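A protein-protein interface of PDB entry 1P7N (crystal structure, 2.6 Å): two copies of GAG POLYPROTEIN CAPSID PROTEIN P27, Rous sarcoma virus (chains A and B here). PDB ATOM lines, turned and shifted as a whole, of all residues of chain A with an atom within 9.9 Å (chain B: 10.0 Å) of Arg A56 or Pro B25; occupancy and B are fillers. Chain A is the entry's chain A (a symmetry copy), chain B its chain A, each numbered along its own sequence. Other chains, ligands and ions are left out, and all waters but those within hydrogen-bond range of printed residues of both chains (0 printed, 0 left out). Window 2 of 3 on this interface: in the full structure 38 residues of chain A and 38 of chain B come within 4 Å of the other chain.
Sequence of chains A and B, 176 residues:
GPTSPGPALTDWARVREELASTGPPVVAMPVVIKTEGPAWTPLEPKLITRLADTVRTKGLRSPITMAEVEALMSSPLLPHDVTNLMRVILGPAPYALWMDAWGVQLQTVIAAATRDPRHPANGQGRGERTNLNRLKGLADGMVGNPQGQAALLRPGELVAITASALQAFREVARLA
Among the printed residues, pairs that only touch across the chains: Thr A49 with Glu B18 (3.7 Å), Arg A56 with Pro B25 (3.9 Å), Arg A56 with Val B26 (3.6 Å) and Val A88 with Leu B19 (3.5 Å).
Of the 24 printed residues of chain A, 3 touch a printed residue of chain B. Printed residues of chain A that touch a printed residue of chain B: Thr A49, Arg A56 and Val A88. Hydrophobic or aromatic side chains of chain A within 4 Å of the printed part of chain B: Val A88. Along chain A the printed residues that touch a printed residue of chain B span positions 49 to 88. Of the 13 printed residues of chain B, 6 touch a printed residue of chain A. Among the printed residues, 6 pairs touch across the chains.
No position is printed for both chains.
The backbone carbonyl oxygen (O) of Glu B18 lies within hydrogen-bond range of the side-chain hydroxyl (OG) of Ser B21, at 3.0 Å.
Of the printed residues of chain B, Thr A49 touches Glu B18. No residue of chain B comes within 4 Å of Ala A52. No residue of chain B comes within 4 Å of Val A55. No residue of chain B comes within 4 Å of Gly A59. Arg B16 touches none of the printed residues of chain A. Printed residues of chain A within 4 Å of Glu B18: Thr A49. Of the printed residues of chain A, Leu B19 touches Val A88 (3.5 Å). Gly B23 touches one residue of chain A. Pro B25 touches just one residue of chain A: Arg A56. Val B26 touches just one residue of chain A: Arg A56. Met B29 touches none of the printed residues of chain A. The nearest residue of chain B that does not touch Arg A56 is Pro B24 (4.2 Å). The nearest residue of chain A that does not touch Pro B25 is Pro A92 (7.1 Å). The nearest printed residue of chain A that does not touch Thr B22 is Asp A53 (4.9 Å).
The backbone carbonyl oxygen (O) of Gly B23 lies within hydrogen-bond range of the guanidinium group (NH2) of Arg A56. The backbone carbonyl oxygen (O) of Thr B22 sits at hydrogen-bond distance from the guanidinium group (NH1) of Arg A56 (3.4 Å).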
ATOM      1  N   ILE A  48      -2.257   8.281 -14.184  1.00  0.00           N
ATOM      2  CA  ILE A  48      -2.068   9.161 -13.027  1.00  0.00           C
ATOM      3  C   ILE A  48      -3.085   8.882 -11.926  1.00  0.00           C
ATOM      4  O   ILE A  48      -2.753   8.904 -10.739  1.00  0.00           O
ATOM      5  CB  ILE A  48      -2.156  10.648 -13.418  1.00  0.00           C
ATOM      6  CG1 ILE A  48      -0.896  11.055 -14.193  1.00  0.00           C
ATOM      7  CG2 ILE A  48      -2.288  11.500 -12.179  1.00  0.00           C
ATOM      8  CD1 ILE A  48      -0.937  12.446 -14.767  1.00  0.00           C
ATOM      9  N   THR A  49      -4.324   8.610 -12.319  1.00  0.00           N
ATOM     10  CA  THR A  49      -5.374   8.318 -11.352  1.00  0.00           C
ATOM     11  C   THR A  49      -5.036   7.049 -10.583  1.00  0.00           C
ATOM     12  O   THR A  49      -5.094   7.025  -9.358  1.00  0.00           O
ATOM     13  CB  THR A  49      -6.710   8.113 -12.045  1.00  0.00           C
ATOM     14  OG1 THR A  49      -6.686   6.866 -12.754  1.00  0.00           O
ATOM     15  CG2 THR A  49      -6.965   9.244 -13.026  1.00  0.00           C
ATOM     16  N   ARG A  50      -4.676   5.993 -11.302  1.00  0.00           N
ATOM     17  CA  ARG A  50      -4.329   4.735 -10.654  1.00  0.00           C
ATOM     18  C   ARG A  50      -3.133   4.929  -9.731  1.00  0.00           C
ATOM     19  O   ARG A  50      -2.982   4.214  -8.750  1.00  0.00           O
ATOM     20  CB  ARG A  50      -4.018   3.664 -11.697  1.00  0.00           C
ATOM     21  CG  ARG A  50      -2.805   3.978 -12.552  1.00  0.00           C
ATOM     22  CD  ARG A  50      -2.438   2.785 -13.394  1.00  0.00           C
ATOM     23  NE  ARG A  50      -2.379   1.575 -12.575  1.00  0.00           N
ATOM     24  CZ  ARG A  50      -2.296   0.344 -13.070  1.00  0.00           C
ATOM     25  NH1 ARG A  50      -2.263   0.155 -14.387  1.00  0.00           N
ATOM     26  NH2 ARG A  50      -2.247  -0.697 -12.249  1.00  0.00           N
ATOM     27  N   LEU A  51      -2.264   5.882 -10.040  1.00  0.00           N
ATOM     28  CA  LEU A  51      -1.146   6.115  -9.138  1.00  0.00           C
ATOM     29  C   LEU A  51      -1.706   6.744  -7.879  1.00  0.00           C
ATOM     30  O   LEU A  51      -1.277   6.427  -6.777  1.00  0.00           O
ATOM     31  CB  LEU A  51      -0.103   7.051  -9.742  1.00  0.00           C
ATOM     32  CG  LEU A  51       0.966   7.469  -8.723  1.00  0.00           C
ATOM     33  CD1 LEU A  51       1.561   6.258  -8.041  1.00  0.00           C
ATOM     34  CD2 LEU A  51       2.050   8.255  -9.424  1.00  0.00           C
ATOM     35  N   ALA A  52      -2.670   7.643  -8.052  1.00  0.00           N
ATOM     36  CA  ALA A  52      -3.302   8.301  -6.919  1.00  0.00           C
ATOM     37  C   ALA A  52      -3.959   7.204  -6.091  1.00  0.00           C
ATOM     38  O   ALA A  52      -3.756   7.121  -4.875  1.00  0.00           O
ATOM     39  CB  ALA A  52      -4.340   9.302  -7.402  1.00  0.00           C
ATOM     40  N   ASP A  53      -4.738   6.356  -6.760  1.00  0.00           N
ATOM     41  CA  ASP A  53      -5.402   5.247  -6.084  1.00  0.00           C
ATOM     42  C   ASP A  53      -4.390   4.427  -5.296  1.00  0.00           C
ATOM     43  O   ASP A  53      -4.578   4.166  -4.112  1.00  0.00           O
ATOM     44  CB  ASP A  53      -6.116   4.326  -7.089  1.00  0.00           C
ATOM     45  CG  ASP A  53      -7.481   4.855  -7.511  1.00  0.00           C
ATOM     46  OD1 ASP A  53      -8.198   5.425  -6.657  1.00  0.00           O
ATOM     47  OD2 ASP A  53      -7.852   4.685  -8.696  1.00  0.00           O
ATOM     48  N   THR A  54      -3.315   4.024  -5.956  1.00  0.00           N
ATOM     49  CA  THR A  54      -2.299   3.233  -5.298  1.00  0.00           C
ATOM     50  C   THR A  54      -1.709   3.992  -4.120  1.00  0.00           C
ATOM     51  O   THR A  54      -1.515   3.431  -3.047  1.00  0.00           O
ATOM     52  CB  THR A  54      -1.179   2.826  -6.288  1.00  0.00           C
ATOM     53  OG1 THR A  54      -1.750   2.075  -7.373  1.00  0.00           O
ATOM     54  CG2 THR A  54      -0.133   1.960  -5.591  1.00  0.00           C
ATOM     55  N   VAL A  55      -1.430   5.276  -4.297  1.00  0.00           N
ATOM     56  CA  VAL A  55      -0.868   6.026  -3.185  1.00  0.00           C
ATOM     57  C   VAL A  55      -1.889   6.142  -2.068  1.00  0.00           C
ATOM     58  O   VAL A  55      -1.534   6.150  -0.887  1.00  0.00           O
ATOM     59  CB  VAL A  55      -0.414   7.427  -3.601  1.00  0.00           C
ATOM     60  CG1 VAL A  55      -0.021   8.217  -2.361  1.00  0.00           C
ATOM     61  CG2 VAL A  55       0.785   7.326  -4.546  1.00  0.00           C
ATOM     62  N   ARG A  56      -3.161   6.236  -2.438  1.00  0.00           N
ATOM     63  CA  ARG A  56      -4.217   6.327  -1.442  1.00  0.00           C
ATOM     64  C   ARG A  56      -4.210   5.031  -0.636  1.00  0.00           C
ATOM     65  O   ARG A  56      -3.678   4.980   0.474  1.00  0.00           O
ATOM     66  CB  ARG A  56      -5.583   6.522  -2.117  1.00  0.00           C
ATOM     67  CG  ARG A  56      -5.958   7.977  -2.423  1.00  0.00           C
ATOM     68  CD  ARG A  56      -7.429   8.093  -2.848  1.00  0.00           C
ATOM     69  NE  ARG A  56      -7.940   9.461  -2.711  1.00  0.00           N
ATOM     70  CZ  ARG A  56      -9.208   9.827  -2.915  1.00  0.00           C
ATOM     71  NH1 ARG A  56     -10.123   8.932  -3.272  1.00  0.00           N
ATOM     72  NH2 ARG A  56      -9.565  11.099  -2.762  1.00  0.00           N
ATOM     73  N   THR A  57      -4.790   3.984  -1.217  1.00  0.00           N
ATOM     74  CA  THR A  57      -4.872   2.667  -0.591  1.00  0.00           C
ATOM     75  C   THR A  57      -3.548   2.145  -0.014  1.00  0.00           C
ATOM     76  O   THR A  57      -3.268   2.348   1.164  1.00  0.00           O
ATOM     77  CB  THR A  57      -5.447   1.630  -1.591  1.00  0.00           C
ATOM     78  OG1 THR A  57      -4.727   1.690  -2.828  1.00  0.00           O
ATOM     79  CG2 THR A  57      -6.907   1.926  -1.874  1.00  0.00           C
ATOM     80  N   LYS A  58      -2.737   1.484  -0.839  1.00  0.00           N
ATOM     81  CA  LYS A  58      -1.453   0.919  -0.394  1.00  0.00           C
ATOM     82  C   LYS A  58      -0.580   1.806   0.494  1.00  0.00           C
ATOM     83  O   LYS A  58       0.384   1.322   1.089  1.00  0.00           O
ATOM     84  CB  LYS A  58      -0.609   0.470  -1.590  1.00  0.00           C
ATOM     85  CG  LYS A  58      -1.189  -0.679  -2.411  1.00  0.00           C
ATOM     86  CD  LYS A  58      -1.422  -1.946  -1.598  1.00  0.00           C
ATOM     87  CE  LYS A  58      -2.803  -1.953  -0.959  1.00  0.00           C
ATOM     88  NZ  LYS A  58      -3.033  -3.192  -0.155  1.00  0.00           N
ATOM     89  N   GLY A  59      -0.897   3.094   0.582  1.00  0.00           N
ATOM     90  CA  GLY A  59      -0.093   3.973   1.410  1.00  0.00           C
ATOM     91  C   GLY A  59       0.860   4.848   0.620  1.00  0.00           C
ATOM     92  O   GLY A  59       0.647   5.106  -0.558  1.00  0.00           O
ATOM     93  N   LEU A  60       1.923   5.300   1.272  1.00  0.00           N
ATOM     94  CA  LEU A  60       2.903   6.170   0.637  1.00  0.00           C
ATOM     95  C   LEU A  60       4.293   5.611   0.891  1.00  0.00           C
ATOM     96  O   LEU A  60       5.143   5.606   0.001  1.00  0.00           O
ATOM     97  CB  LEU A  60       2.774   7.587   1.214  1.00  0.00           C
ATOM     98  CG  LEU A  60       3.496   8.774   0.560  1.00  0.00           C
ATOM     99  CD1 LEU A  60       5.006   8.637   0.746  1.00  0.00           C
ATOM    100  CD2 LEU A  60       3.118   8.860  -0.921  1.00  0.00           C
ATOM    101  N   ARG A  61       4.526   5.154   2.119  1.00  0.00           N
ATOM    102  CA  ARG A  61       5.813   4.564   2.469  1.00  0.00           C
ATOM    103  C   ARG A  61       5.848   3.183   1.827  1.00  0.00           C
ATOM    104  O   ARG A  61       6.863   2.490   1.866  1.00  0.00           O
ATOM    105  CB  ARG A  61       5.962   4.419   3.989  1.00  0.00           C
ATOM    106  CG  ARG A  61       6.403   5.676   4.728  1.00  0.00           C
ATOM    107  CD  ARG A  61       6.672   5.378   6.207  1.00  0.00           C
ATOM    108  NE  ARG A  61       7.635   4.286   6.401  1.00  0.00           N
ATOM    109  CZ  ARG A  61       8.939   4.359   6.133  1.00  0.00           C
ATOM    110  NH1 ARG A  61       9.465   5.479   5.655  1.00  0.00           N
ATOM    111  NH2 ARG A  61       9.725   3.307   6.341  1.00  0.00           N
ATOM    112  N   SER A  62       4.715   2.796   1.248  1.00  0.00           N
ATOM    113  CA  SER A  62       4.572   1.510   0.587  1.00  0.00           C
ATOM    114  C   SER A  62       5.559   1.310  -0.553  1.00  0.00           C
ATOM    115  O   SER A  62       5.814   2.225  -1.339  1.00  0.00           O
ATOM    116  CB  SER A  62       3.162   1.359   0.034  1.00  0.00           C
ATOM    117  OG  SER A  62       3.114   0.263  -0.862  1.00  0.00           O
ATOM    118  N   ILE A  64       5.109  -0.546  -3.076  1.00  0.00           N
ATOM    119  CA  ILE A  64       4.326  -0.581  -4.304  1.00  0.00           C
ATOM    120  C   ILE A  64       4.268   0.811  -4.885  1.00  0.00           C
ATOM    121  O   ILE A  64       4.419   1.020  -6.085  1.00  0.00           O
ATOM    122  CB  ILE A  64       2.877  -1.030  -4.047  1.00  0.00           C
ATOM    123  CG1 ILE A  64       2.871  -2.387  -3.334  1.00  0.00           C
ATOM    124  CG2 ILE A  64       2.105  -1.065  -5.381  1.00  0.00           C
ATOM    125  CD1 ILE A  64       1.490  -2.948  -3.082  1.00  0.00           C
ATOM    126  N   THR A  65       4.015   1.775  -4.020  1.00  0.00           N
ATOM    127  CA  THR A  65       3.942   3.143  -4.454  1.00  0.00           C
ATOM    128  C   THR A  65       5.292   3.541  -5.029  1.00  0.00           C
ATOM    129  O   THR A  65       5.371   4.038  -6.153  1.00  0.00           O
ATOM    130  CB  THR A  65       3.538   4.029  -3.271  1.00  0.00           C
ATOM    131  OG1 THR A  65       2.136   3.836  -3.024  1.00  0.00           O
ATOM    132  CG2 THR A  65       3.850   5.519  -3.541  1.00  0.00           C
ATOM    133  N   GLU A  68       5.707   1.958  -8.387  1.00  0.00           N
ATOM    134  CA  GLU A  68       4.876   2.577  -9.408  1.00  0.00           C
ATOM    135  C   GLU A  68       5.285   4.022  -9.758  1.00  0.00           C
ATOM    136  O   GLU A  68       5.123   4.444 -10.905  1.00  0.00           O
ATOM    137  CB  GLU A  68       3.410   2.501  -8.975  1.00  0.00           C
ATOM    138  CG  GLU A  68       2.422   2.197 -10.107  1.00  0.00           C
ATOM    139  CD  GLU A  68       0.959   2.400  -9.682  1.00  0.00           C
ATOM    140  OE1 GLU A  68       0.072   2.558 -10.563  1.00  0.00           O
ATOM    141  OE2 GLU A  68       0.699   2.395  -8.459  1.00  0.00           O
ATOM    142  N   VAL A  69       5.824   4.773  -8.795  1.00  0.00           N
ATOM    143  CA  VAL A  69       6.263   6.151  -9.062  1.00  0.00           C
ATOM    144  C   VAL A  69       7.566   6.087  -9.830  1.00  0.00           C
ATOM    145  O   VAL A  69       7.738   6.747 -10.852  1.00  0.00           O
ATOM    146  CB  VAL A  69       6.525   6.973  -7.758  1.00  0.00           C
ATOM    147  CG1 VAL A  69       7.139   8.314  -8.111  1.00  0.00           C
ATOM    148  CG2 VAL A  69       5.216   7.198  -6.984  1.00  0.00           C
ATOM    149  N   VAL A  88      -0.500  15.978  -6.623  1.00  0.00           N
ATOM    150  CA  VAL A  88      -1.604  15.030  -6.568  1.00  0.00           C
ATOM    151  C   VAL A  88      -1.358  13.814  -5.681  1.00  0.00           C
ATOM    152  O   VAL A  88      -2.218  13.432  -4.908  1.00  0.00           O
ATOM    153  CB  VAL A  88      -1.964  14.532  -7.958  1.00  0.00           C
ATOM    154  CG1 VAL A  88      -3.237  13.717  -7.883  1.00  0.00           C
ATOM    155  CG2 VAL A  88      -2.126  15.715  -8.911  1.00  0.00           C
ATOM    156  N   ILE A  89      -0.180  13.214  -5.776  1.00  0.00           N
ATOM    157  CA  ILE A  89       0.115  12.032  -4.975  1.00  0.00           C
ATOM    158  C   ILE A  89       0.496  12.347  -3.539  1.00  0.00           C
ATOM    159  O   ILE A  89       0.026  11.681  -2.619  1.00  0.00           O
ATOM    160  CB  ILE A  89       1.254  11.188  -5.607  1.00  0.00           C
ATOM    161  CG1 ILE A  89       2.519  12.033  -5.729  1.00  0.00           C
ATOM    162  CG2 ILE A  89       0.829  10.667  -6.977  1.00  0.00           C
ATOM    163  CD1 ILE A  89       3.710  11.267  -6.226  1.00  0.00           C
ATOM    164  N   LEU A  90       1.339  13.364  -3.355  1.00  0.00           N
ATOM    165  CA  LEU A  90       1.823  13.776  -2.037  1.00  0.00           C
ATOM    166  C   LEU A  90       0.838  14.444  -1.088  1.00  0.00           C
ATOM    167  O   LEU A  90       0.928  14.259   0.124  1.00  0.00           O
ATOM    168  CB  LEU A  90       3.015  14.711  -2.188  1.00  0.00           C
ATOM    169  CG  LEU A  90       4.297  14.099  -2.739  1.00  0.00           C
ATOM    170  CD1 LEU A  90       5.367  15.170  -2.775  1.00  0.00           C
ATOM    171  CD2 LEU A  90       4.743  12.927  -1.875  1.00  0.00           C
ATOM    172  N   GLY A  91      -0.087  15.234  -1.615  1.00  0.00           N
ATOM    173  CA  GLY A  91      -1.015  15.920  -0.737  1.00  0.00           C
ATOM    174  C   GLY A  91      -0.398  17.226  -0.258  1.00  0.00           C
ATOM    175  O   GLY A  91       0.830  17.368  -0.261  1.00  0.00           O
ATOM    176  N   PRO A  92      -1.220  18.185   0.206  1.00  0.00           N
ATOM    177  CA  PRO A  92      -0.788  19.502   0.689  1.00  0.00           C
ATOM    178  C   PRO A  92       0.442  19.531   1.584  1.00  0.00           C
ATOM    179  O   PRO A  92       1.426  20.203   1.280  1.00  0.00           O
ATOM    180  CB  PRO A  92      -2.030  20.030   1.407  1.00  0.00           C
ATOM    181  CG  PRO A  92      -3.164  19.377   0.663  1.00  0.00           C
ATOM    182  CD  PRO A  92      -2.646  17.967   0.530  1.00  0.00           C
ATOM    183  N   ARG B  16      -7.796  16.477 -13.190  1.00  0.00           N
ATOM    184  CA  ARG B  16      -8.591  17.204 -12.206  1.00  0.00           C
ATOM    185  C   ARG B  16      -9.940  16.505 -12.066  1.00  0.00           C
ATOM    186  O   ARG B  16     -10.259  15.946 -11.020  1.00  0.00           O
ATOM    187  CB  ARG B  16      -8.788  18.669 -12.637  1.00  0.00           C
ATOM    188  CG  ARG B  16      -9.717  19.484 -11.738  1.00  0.00           C
ATOM    189  CD  ARG B  16      -9.811  20.957 -12.153  1.00  0.00           C
ATOM    190  NE  ARG B  16      -8.773  21.764 -11.508  1.00  0.00           N
ATOM    191  CZ  ARG B  16      -8.798  22.164 -10.234  1.00  0.00           C
ATOM    192  NH1 ARG B  16      -9.827  21.850  -9.444  1.00  0.00           N
ATOM    193  NH2 ARG B  16      -7.770  22.848  -9.733  1.00  0.00           N
ATOM    194  N   GLU B  18     -11.144  13.632 -12.868  1.00  0.00           N
ATOM    195  CA  GLU B  18     -11.104  12.281 -12.308  1.00  0.00           C
ATOM    196  C   GLU B  18     -11.096  12.356 -10.785  1.00  0.00           C
ATOM    197  O   GLU B  18     -12.102  12.098 -10.130  1.00  0.00           O
ATOM    198  CB  GLU B  18      -9.848  11.545 -12.782  1.00  0.00           C
ATOM    199  CG  GLU B  18      -9.793  11.294 -14.279  1.00  0.00           C
ATOM    200  CD  GLU B  18     -10.616  10.093 -14.710  1.00  0.00           C
ATOM    201  OE1 GLU B  18     -11.554   9.720 -13.975  1.00  0.00           O
ATOM    202  OE2 GLU B  18     -10.327   9.530 -15.791  1.00  0.00           O
ATOM    203  N   LEU B  19      -9.946  12.718 -10.236  1.00  0.00           N
ATOM    204  CA  LEU B  19      -9.764  12.839  -8.799  1.00  0.00           C
ATOM    205  C   LEU B  19     -11.013  13.356  -8.088  1.00  0.00           C
ATOM    206  O   LEU B  19     -11.350  12.889  -7.002  1.00  0.00           O
ATOM    207  CB  LEU B  19      -8.596  13.781  -8.512  1.00  0.00           C
ATOM    208  CG  LEU B  19      -7.372  13.568  -9.398  1.00  0.00           C
ATOM    209  CD1 LEU B  19      -6.343  14.658  -9.136  1.00  0.00           C
ATOM    210  CD2 LEU B  19      -6.797  12.192  -9.139  1.00  0.00           C
ATOM    211  N   ALA B  20     -11.691  14.319  -8.706  1.00  0.00           N
ATOM    212  CA  ALA B  20     -12.897  14.911  -8.130  1.00  0.00           C
ATOM    213  C   ALA B  20     -14.022  13.898  -7.995  1.00  0.00           C
ATOM    214  O   ALA B  20     -14.514  13.640  -6.892  1.00  0.00           O
ATOM    215  CB  ALA B  20     -13.362  16.083  -8.983  1.00  0.00           C
ATOM    216  N   SER B  21     -14.425  13.324  -9.123  1.00  0.00           N
ATOM    217  CA  SER B  21     -15.500  12.340  -9.134  1.00  0.00           C
ATOM    218  C   SER B  21     -15.138  11.048  -8.391  1.00  0.00           C
ATOM    219  O   SER B  21     -15.711   9.991  -8.664  1.00  0.00           O
ATOM    220  CB  SER B  21     -15.897  12.013 -10.581  1.00  0.00           C
ATOM    221  OG  SER B  21     -14.825  11.417 -11.294  1.00  0.00           O
ATOM    222  N   THR B  22     -14.195  11.134  -7.452  1.00  0.00           N
ATOM    223  CA  THR B  22     -13.774   9.969  -6.674  1.00  0.00           C
ATOM    224  C   THR B  22     -13.123  10.368  -5.344  1.00  0.00           C
ATOM    225  O   THR B  22     -11.992  10.852  -5.317  1.00  0.00           O
ATOM    226  CB  THR B  22     -12.756   9.092  -7.463  1.00  0.00           C
ATOM    227  OG1 THR B  22     -13.312   8.718  -8.731  1.00  0.00           O
ATOM    228  CG2 THR B  22     -12.418   7.825  -6.677  1.00  0.00           C
ATOM    229  N   GLY B  23     -13.844  10.163  -4.245  1.00  0.00           N
ATOM    230  CA  GLY B  23     -13.306  10.479  -2.931  1.00  0.00           C
ATOM    231  C   GLY B  23     -13.006  11.943  -2.679  1.00  0.00           C
ATOM    232  O   GLY B  23     -12.454  12.618  -3.547  1.00  0.00           O
ATOM    233  N   PRO B  24     -13.380  12.466  -1.497  1.00  0.00           N
ATOM    234  CA  PRO B  24     -13.154  13.867  -1.116  1.00  0.00           C
ATOM    235  C   PRO B  24     -11.845  14.262  -0.405  1.00  0.00           C
ATOM    236  O   PRO B  24     -11.346  15.361  -0.649  1.00  0.00           O
ATOM    237  CB  PRO B  24     -14.374  14.196  -0.246  1.00  0.00           C
ATOM    238  CG  PRO B  24     -15.399  13.182  -0.666  1.00  0.00           C
ATOM    239  CD  PRO B  24     -14.557  11.943  -0.787  1.00  0.00           C
ATOM    240  N   PRO B  25     -11.275  13.386   0.467  1.00  0.00           N
ATOM    241  CA  PRO B  25     -10.029  13.706   1.192  1.00  0.00           C
ATOM    242  C   PRO B  25      -9.293  14.879   0.554  1.00  0.00           C
ATOM    243  O   PRO B  25      -9.520  16.040   0.907  1.00  0.00           O
ATOM    244  CB  PRO B  25      -9.257  12.395   1.121  1.00  0.00           C
ATOM    245  CG  PRO B  25     -10.350  11.404   1.348  1.00  0.00           C
ATOM    246  CD  PRO B  25     -11.495  11.925   0.473  1.00  0.00           C
ATOM    247  N   VAL B  26      -8.391  14.573  -0.366  1.00  0.00           N
ATOM    248  CA  VAL B  26      -7.711  15.617  -1.105  1.00  0.00           C
ATOM    249  C   VAL B  26      -8.524  15.428  -2.378  1.00  0.00           C
ATOM    250  O   VAL B  26      -9.504  14.681  -2.350  1.00  0.00           O
ATOM    251  CB  VAL B  26      -6.235  15.279  -1.349  1.00  0.00           C
ATOM    252  CG1 VAL B  26      -5.516  16.497  -1.919  1.00  0.00           C
ATOM    253  CG2 VAL B  26      -5.582  14.826  -0.047  1.00  0.00           C
ATOM    254  N   VAL B  27      -8.166  16.070  -3.482  1.00  0.00           N
ATOM    255  CA  VAL B  27      -8.953  15.868  -4.700  1.00  0.00           C
ATOM    256  C   VAL B  27      -8.335  16.385  -5.995  1.00  0.00           C
ATOM    257  O   VAL B  27      -7.123  16.291  -6.220  1.00  0.00           O
ATOM    258  CB  VAL B  27     -10.380  16.495  -4.571  1.00  0.00           C
ATOM    259  CG1 VAL B  27     -11.418  15.400  -4.313  1.00  0.00           C
ATOM    260  CG2 VAL B  27     -10.403  17.547  -3.448  1.00  0.00           C
ATOM    261  N   ALA B  28      -9.207  16.905  -6.855  1.00  0.00           N
ATOM    262  CA  ALA B  28      -8.819  17.457  -8.136  1.00  0.00           C
ATOM    263  C   ALA B  28      -8.037  18.718  -7.868  1.00  0.00           C
ATOM    264  O   ALA B  28      -8.501  19.816  -8.158  1.00  0.00           O
ATOM    265  CB  ALA B  28     -10.054  17.781  -8.947  1.00  0.00           C
ATOM    266  N   MET B  29      -6.847  18.578  -7.309  1.00  0.00           N
ATOM    267  CA  MET B  29      -6.074  19.761  -7.036  1.00  0.00           C
ATOM    268  C   MET B  29      -4.767  19.975  -7.796  1.00  0.00           C
ATOM    269  O   MET B  29      -3.813  20.528  -7.251  1.00  0.00           O
ATOM    270  CB  MET B  29      -5.867  19.904  -5.527  1.00  0.00           C
ATOM    271  CG  MET B  29      -6.036  18.633  -4.736  1.00  0.00           C
ATOM    272  SD  MET B  29      -4.568  17.669  -4.906  1.00  0.00           S
ATOM    273  CE  MET B  29      -3.499  18.561  -3.713  1.00  0.00           C
